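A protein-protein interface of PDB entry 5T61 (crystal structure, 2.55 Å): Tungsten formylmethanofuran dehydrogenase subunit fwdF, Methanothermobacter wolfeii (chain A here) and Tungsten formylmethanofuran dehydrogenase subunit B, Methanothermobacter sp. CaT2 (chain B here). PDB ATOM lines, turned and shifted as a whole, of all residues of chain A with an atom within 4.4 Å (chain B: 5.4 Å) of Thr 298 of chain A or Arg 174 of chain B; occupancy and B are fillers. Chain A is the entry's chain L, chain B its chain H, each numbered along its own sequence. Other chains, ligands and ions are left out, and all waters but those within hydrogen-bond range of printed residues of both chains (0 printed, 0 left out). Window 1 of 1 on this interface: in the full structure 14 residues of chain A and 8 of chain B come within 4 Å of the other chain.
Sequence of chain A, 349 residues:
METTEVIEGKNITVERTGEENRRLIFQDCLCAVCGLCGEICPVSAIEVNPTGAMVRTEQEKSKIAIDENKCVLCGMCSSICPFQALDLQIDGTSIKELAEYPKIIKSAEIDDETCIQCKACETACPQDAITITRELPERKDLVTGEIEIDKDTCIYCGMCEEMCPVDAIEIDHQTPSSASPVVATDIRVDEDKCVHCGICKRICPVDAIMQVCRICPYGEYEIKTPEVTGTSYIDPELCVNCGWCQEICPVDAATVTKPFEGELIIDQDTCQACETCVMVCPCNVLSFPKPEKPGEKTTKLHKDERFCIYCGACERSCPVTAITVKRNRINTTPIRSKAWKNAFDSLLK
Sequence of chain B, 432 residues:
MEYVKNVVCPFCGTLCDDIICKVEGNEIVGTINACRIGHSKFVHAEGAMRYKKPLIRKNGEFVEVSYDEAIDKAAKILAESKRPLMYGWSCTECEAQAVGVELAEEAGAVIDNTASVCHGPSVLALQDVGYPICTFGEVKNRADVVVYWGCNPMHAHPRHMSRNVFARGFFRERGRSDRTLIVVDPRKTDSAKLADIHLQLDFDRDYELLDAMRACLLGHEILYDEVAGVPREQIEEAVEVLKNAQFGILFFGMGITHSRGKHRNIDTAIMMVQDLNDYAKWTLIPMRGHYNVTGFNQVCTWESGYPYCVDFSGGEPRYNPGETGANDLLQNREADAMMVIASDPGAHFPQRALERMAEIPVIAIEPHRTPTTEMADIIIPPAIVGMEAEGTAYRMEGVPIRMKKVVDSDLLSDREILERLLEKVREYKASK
O of Thr 299 of chain A lies within hydrogen-bond range of NH2 of Arg 174 of chain B, 3.0 Å away.
The backbone carbonyl oxygen (O) of Thr 298 of chain A sits close to the side-chain carboxylate (OE2) of Glu 173 of chain B, at 3.4 Å.
The guanidinium group of Arg 174 of chain B sits at hydrogen-bond distance from the backbone carbonyl oxygen of Pro 289 of chain A (3.1 Å).
The backbone carbonyl oxygen (O) of Lys 300 of chain A sits at hydrogen-bond distance from the guanidinium group (NE) of Arg 174 of chain B (2.9 Å).
OG1 of Thr 298 of chain A is in hydrogen-bond range of NH2 of Arg 174 of chain B (2.9 Å).
Arg 174 of chain B touches Ala 273 of chain A (CB to CB, 3.5 Å).
CD of Arg 174 of chain B touches CG of Phe 288 of chain A (3.4 Å).
CE2 of Phe 288 of chain A touches OG of Ser 177 of chain B, 3.7 Å away.
CG of Pro 291 of chain A touches NH1 of Arg 172 of chain B, at 3.5 Å.
CB of Lys 300 of chain A touches OE2 of Glu 173 of chain B, at 3.7 Å.
Of the 8 printed residues of chain B, 4 touch a printed residue of chain A.
Of the 9 printed residues of chain A, 7 touch a printed residue of chain B.
Hydrophobic or aromatic side chains of chain A that line the printed part of chain B: Ala 273, Phe 288, Pro 289 and Pro 291.
Among the printed residues, no Asp or Glu carboxylate lies within 4 Å of a Lys or Arg side-chain nitrogen of the other chain.
The side-chain carboxylate (OD2) of Asp 178 of chain B lies within hydrogen-bond range of the backbone NH (N) of Glu 173 of chain B (3.3 Å).
NH1 of Arg 174 of chain B lies within salt-bridge range of OD1 of Asp 178 of chain B (2.9 Å).
The backbone carbonyl oxygen (O) of Pro 289 of chain A is in hydrogen-bond range of the side-chain hydroxyl (OG1) of Thr 298 of chain A (3.2 Å).
Printed residues of chain B within 4 Å of Phe 288 of chain A: Arg 174 (3.4 Å) and Ser 177 (3.7 Å).
Of the printed residues of chain B, Pro 289 of chain A touches Arg 174.
Of the printed residues of chain B, Pro 291 of chain A touches Arg 172 (3.5 Å).
Of chain B, only Glu 173 (3.4 Å) and Arg 174 (2.9 Å) come within 4 Å of Thr 298 of chain A.
Of the printed residues of chain B, Lys 300 of chain A touches Glu 173 (3.7 Å) and Arg 174 (2.9 Å).
Arg 168 of chain B touches none of the printed residues of chain A.
Arg 174 of chain B touches just these residues of chain A: Ala 273 (3.5 Å), Phe 288 (3.4 Å), Pro 289 (3.1 Å), Thr 298 (2.9 Å), Thr 299 (3.0 Å) and Lys 300 (2.9 Å).
The nearest printed residue of chain B that does not touch Thr 298 of chain A is Asp 178 of chain B (6.5 Å).
The nearest printed residue of chain A that does not touch Arg 174 of chain B is Lys 290 of chain A (5.0 Å).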
ATOM      1  N   ALA A 273       8.046  14.558  26.871  1.00  0.00           N
ATOM      2  CA  ALA A 273       7.109  13.517  26.450  1.00  0.00           C
ATOM      3  C   ALA A 273       7.562  12.123  26.877  1.00  0.00           C
ATOM      4  O   ALA A 273       7.457  11.161  26.112  1.00  0.00           O
ATOM      5  CB  ALA A 273       6.877  13.570  24.940  1.00  0.00           C
ATOM      6  N   PHE A 288      -1.527  12.120  24.731  1.00  0.00           N
ATOM      7  CA  PHE A 288      -0.679  12.428  23.584  1.00  0.00           C
ATOM      8  C   PHE A 288      -1.548  12.325  22.340  1.00  0.00           C
ATOM      9  O   PHE A 288      -1.730  11.225  21.796  1.00  0.00           O
ATOM     10  CB  PHE A 288       0.511  11.469  23.492  1.00  0.00           C
ATOM     11  CG  PHE A 288       1.560  11.680  24.546  1.00  0.00           C
ATOM     12  CD1 PHE A 288       1.564  12.822  25.331  1.00  0.00           C
ATOM     13  CD2 PHE A 288       2.576  10.751  24.716  1.00  0.00           C
ATOM     14  CE1 PHE A 288       2.540  13.015  26.288  1.00  0.00           C
ATOM     15  CE2 PHE A 288       3.559  10.946  25.669  1.00  0.00           C
ATOM     16  CZ  PHE A 288       3.541  12.077  26.453  1.00  0.00           C
ATOM     17  N   PRO A 289      -2.144  13.421  21.872  1.00  0.00           N
ATOM     18  CA  PRO A 289      -2.966  13.345  20.653  1.00  0.00           C
ATOM     19  C   PRO A 289      -2.152  12.849  19.463  1.00  0.00           C
ATOM     20  O   PRO A 289      -1.040  13.315  19.212  1.00  0.00           O
ATOM     21  CB  PRO A 289      -3.443  14.787  20.440  1.00  0.00           C
ATOM     22  CG  PRO A 289      -3.091  15.544  21.658  1.00  0.00           C
ATOM     23  CD  PRO A 289      -2.192  14.737  22.530  1.00  0.00           C
ATOM     24  N   LYS A 290      -2.707  11.886  18.743  1.00  0.00           N
ATOM     25  CA  LYS A 290      -2.089  11.443  17.496  1.00  0.00           C
ATOM     26  C   LYS A 290      -2.498  12.377  16.362  1.00  0.00           C
ATOM     27  O   LYS A 290      -3.675  12.740  16.263  1.00  0.00           O
ATOM     28  CB  LYS A 290      -2.478   9.997  17.186  1.00  0.00           C
ATOM     29  CG  LYS A 290      -1.823   9.392  15.946  1.00  0.00           C
ATOM     30  CD  LYS A 290      -2.186   7.914  15.801  1.00  0.00           C
ATOM     31  CE  LYS A 290      -2.106   7.418  14.357  1.00  0.00           C
ATOM     32  NZ  LYS A 290      -2.913   8.241  13.408  1.00  0.00           N
ATOM     33  N   PRO A 291      -1.563  12.800  15.511  1.00  0.00           N
ATOM     34  CA  PRO A 291      -1.930  13.676  14.392  1.00  0.00           C
ATOM     35  C   PRO A 291      -2.863  12.965  13.429  1.00  0.00           C
ATOM     36  O   PRO A 291      -2.716  11.772  13.155  1.00  0.00           O
ATOM     37  CB  PRO A 291      -0.582  14.007  13.738  1.00  0.00           C
ATOM     38  CG  PRO A 291       0.334  12.905  14.163  1.00  0.00           C
ATOM     39  CD  PRO A 291      -0.123  12.489  15.529  1.00  0.00           C
ATOM     40  N   LYS A 297       1.084  18.569  13.027  1.00  0.00           N
ATOM     41  CA  LYS A 297       1.680  18.536  14.345  1.00  0.00           C
ATOM     42  C   LYS A 297       0.598  18.789  15.388  1.00  0.00           C
ATOM     43  O   LYS A 297      -0.425  19.424  15.111  1.00  0.00           O
ATOM     44  CB  LYS A 297       2.780  19.584  14.410  1.00  0.00           C
ATOM     45  CG  LYS A 297       3.734  19.422  13.226  1.00  0.00           C
ATOM     46  CD  LYS A 297       5.035  20.173  13.381  1.00  0.00           C
ATOM     47  CE  LYS A 297       6.112  19.388  14.091  1.00  0.00           C
ATOM     48  NZ  LYS A 297       7.378  20.179  14.021  1.00  0.00           N
ATOM     49  N   THR A 298       0.838  18.285  16.593  1.00  0.00           N
ATOM     50  CA  THR A 298      -0.135  18.318  17.673  1.00  0.00           C
ATOM     51  C   THR A 298       0.551  18.898  18.900  1.00  0.00           C
ATOM     52  O   THR A 298       1.780  18.900  18.998  1.00  0.00           O
ATOM     53  CB  THR A 298      -0.705  16.915  17.967  1.00  0.00           C
ATOM     54  OG1 THR A 298       0.342  16.044  18.412  1.00  0.00           O
ATOM     55  CG2 THR A 298      -1.343  16.322  16.720  1.00  0.00           C
ATOM     56  N   THR A 299      -0.243  19.381  19.849  1.00  0.00           N
ATOM     57  CA  THR A 299       0.343  19.850  21.095  1.00  0.00           C
ATOM     58  C   THR A 299       0.968  18.676  21.833  1.00  0.00           C
ATOM     59  O   THR A 299       0.379  17.593  21.927  1.00  0.00           O
ATOM     60  CB  THR A 299      -0.702  20.544  21.963  1.00  0.00           C
ATOM     61  OG1 THR A 299      -1.331  19.585  22.819  1.00  0.00           O
ATOM     62  CG2 THR A 299      -1.750  21.204  21.089  1.00  0.00           C
ATOM     63  N   LYS A 300       2.186  18.896  22.339  1.00  0.00           N
ATOM     64  CA  LYS A 300       2.988  17.803  22.883  1.00  0.00           C
ATOM     65  C   LYS A 300       2.259  17.079  24.010  1.00  0.00           C
ATOM     66  O   LYS A 300       2.188  15.845  24.021  1.00  0.00           O
ATOM     67  CB  LYS A 300       4.344  18.332  23.358  1.00  0.00           C
ATOM     68  CG  LYS A 300       5.339  17.233  23.691  1.00  0.00           C
ATOM     69  CD  LYS A 300       6.634  17.779  24.261  1.00  0.00           C
ATOM     70  CE  LYS A 300       7.462  18.527  23.242  1.00  0.00           C
ATOM     71  NZ  LYS A 300       8.467  19.391  23.918  1.00  0.00           N
ATOM     72  N   ARG B 168      13.738  11.733  19.426  1.00  0.00           N
ATOM     73  CA  ARG B 168      12.647  12.669  19.184  1.00  0.00           C
ATOM     74  C   ARG B 168      12.910  13.419  17.883  1.00  0.00           C
ATOM     75  O   ARG B 168      13.896  14.155  17.772  1.00  0.00           O
ATOM     76  CB  ARG B 168      12.503  13.637  20.356  1.00  0.00           C
ATOM     77  CG  ARG B 168      12.130  12.964  21.667  1.00  0.00           C
ATOM     78  CD  ARG B 168      12.498  13.845  22.849  1.00  0.00           C
ATOM     79  NE  ARG B 168      12.402  13.134  24.120  1.00  0.00           N
ATOM     80  CZ  ARG B 168      13.335  12.309  24.584  1.00  0.00           C
ATOM     81  NH1 ARG B 168      14.430  12.071  23.872  1.00  0.00           N
ATOM     82  NH2 ARG B 168      13.170  11.708  25.757  1.00  0.00           N
ATOM     83  N   ARG B 172       7.876  13.669  15.071  1.00  0.00           N
ATOM     84  CA  ARG B 172       7.663  12.651  16.098  1.00  0.00           C
ATOM     85  C   ARG B 172       8.371  13.086  17.382  1.00  0.00           C
ATOM     86  O   ARG B 172       9.244  12.398  17.911  1.00  0.00           O
ATOM     87  CB  ARG B 172       8.163  11.282  15.637  1.00  0.00           C
ATOM     88  CG  ARG B 172       7.563  10.780  14.326  1.00  0.00           C
ATOM     89  CD  ARG B 172       6.057  10.595  14.420  1.00  0.00           C
ATOM     90  NE  ARG B 172       5.456  10.348  13.112  1.00  0.00           N
ATOM     91  CZ  ARG B 172       4.234  10.734  12.761  1.00  0.00           C
ATOM     92  NH1 ARG B 172       3.472  11.395  13.621  1.00  0.00           N
ATOM     93  NH2 ARG B 172       3.773  10.457  11.548  1.00  0.00           N
ATOM     94  N   GLU B 173       7.983  14.262  17.882  1.00  0.00           N
ATOM     95  CA  GLU B 173       8.667  14.898  19.003  1.00  0.00           C
ATOM     96  C   GLU B 173       8.548  14.126  20.311  1.00  0.00           C
ATOM     97  O   GLU B 173       9.262  14.458  21.264  1.00  0.00           O
ATOM     98  CB  GLU B 173       8.149  16.326  19.183  1.00  0.00           C
ATOM     99  CG  GLU B 173       6.744  16.428  19.735  1.00  0.00           C
ATOM    100  CD  GLU B 173       6.189  17.830  19.606  1.00  0.00           C
ATOM    101  OE1 GLU B 173       6.983  18.757  19.335  1.00  0.00           O
ATOM    102  OE2 GLU B 173       4.962  18.005  19.767  1.00  0.00           O
ATOM    103  N   ARG B 174       7.680  13.121  20.394  1.00  0.00           N
ATOM    104  CA  ARG B 174       7.573  12.318  21.603  1.00  0.00           C
ATOM    105  C   ARG B 174       8.385  11.033  21.532  1.00  0.00           C
ATOM    106  O   ARG B 174       8.259  10.185  22.420  1.00  0.00           O
ATOM    107  CB  ARG B 174       6.110  11.987  21.912  1.00  0.00           C
ATOM    108  CG  ARG B 174       5.152  13.163  21.788  1.00  0.00           C
ATOM    109  CD  ARG B 174       3.774  12.736  22.251  1.00  0.00           C
ATOM    110  NE  ARG B 174       2.754  13.766  22.088  1.00  0.00           N
ATOM    111  CZ  ARG B 174       1.933  13.837  21.045  1.00  0.00           C
ATOM    112  NH1 ARG B 174       2.008  12.929  20.078  1.00  0.00           N
ATOM    113  NH2 ARG B 174       1.029  14.804  20.969  1.00  0.00           N
ATOM    114  N   GLY B 175       9.221  10.876  20.507  1.00  0.00           N
ATOM    115  CA  GLY B 175      10.065   9.703  20.389  1.00  0.00           C
ATOM    116  C   GLY B 175       9.308   8.393  20.446  1.00  0.00           C
ATOM    117  O   GLY B 175       8.389   8.162  19.653  1.00  0.00           O
ATOM    118  N   ARG B 176       9.705   7.530  21.386  1.00  0.00           N
ATOM    119  CA  ARG B 176       9.156   6.178  21.472  1.00  0.00           C
ATOM    120  C   ARG B 176       7.633   6.185  21.558  1.00  0.00           C
ATOM    121  O   ARG B 176       6.970   5.300  21.003  1.00  0.00           O
ATOM    122  CB  ARG B 176       9.759   5.462  22.684  1.00  0.00           C
ATOM    123  CG  ARG B 176       9.193   4.079  22.960  1.00  0.00           C
ATOM    124  CD  ARG B 176       9.602   3.091  21.880  1.00  0.00           C
ATOM    125  NE  ARG B 176       9.041   1.762  22.111  1.00  0.00           N
ATOM    126  CZ  ARG B 176       7.873   1.353  21.630  1.00  0.00           C
ATOM    127  NH1 ARG B 176       7.131   2.172  20.896  1.00  0.00           N
ATOM    128  NH2 ARG B 176       7.437   0.126  21.887  1.00  0.00           N
ATOM    129  N   SER B 177       7.061   7.181  22.240  1.00  0.00           N
ATOM    130  CA  SER B 177       5.613   7.255  22.405  1.00  0.00           C
ATOM    131  C   SER B 177       4.874   7.527  21.100  1.00  0.00           C
ATOM    132  O   SER B 177       3.676   7.238  21.013  1.00  0.00           O
ATOM    133  CB  SER B 177       5.255   8.336  23.426  1.00  0.00           C
ATOM    134  OG  SER B 177       5.496   7.889  24.746  1.00  0.00           O
ATOM    135  N   ASP B 178       5.549   8.073  20.093  1.00  0.00           N
ATOM    136  CA  ASP B 178       4.919   8.400  18.820  1.00  0.00           C
ATOM    137  C   ASP B 178       5.010   7.277  17.797  1.00  0.00           C
ATOM    138  O   ASP B 178       4.603   7.478  16.648  1.00  0.00           O
ATOM    139  CB  ASP B 178       5.552   9.659  18.227  1.00  0.00           C
ATOM    140  CG  ASP B 178       5.058  10.920  18.884  1.00  0.00           C
ATOM    141  OD1 ASP B 178       4.027  10.857  19.583  1.00  0.00           O
ATOM    142  OD2 ASP B 178       5.705  11.973  18.706  1.00  0.00           O
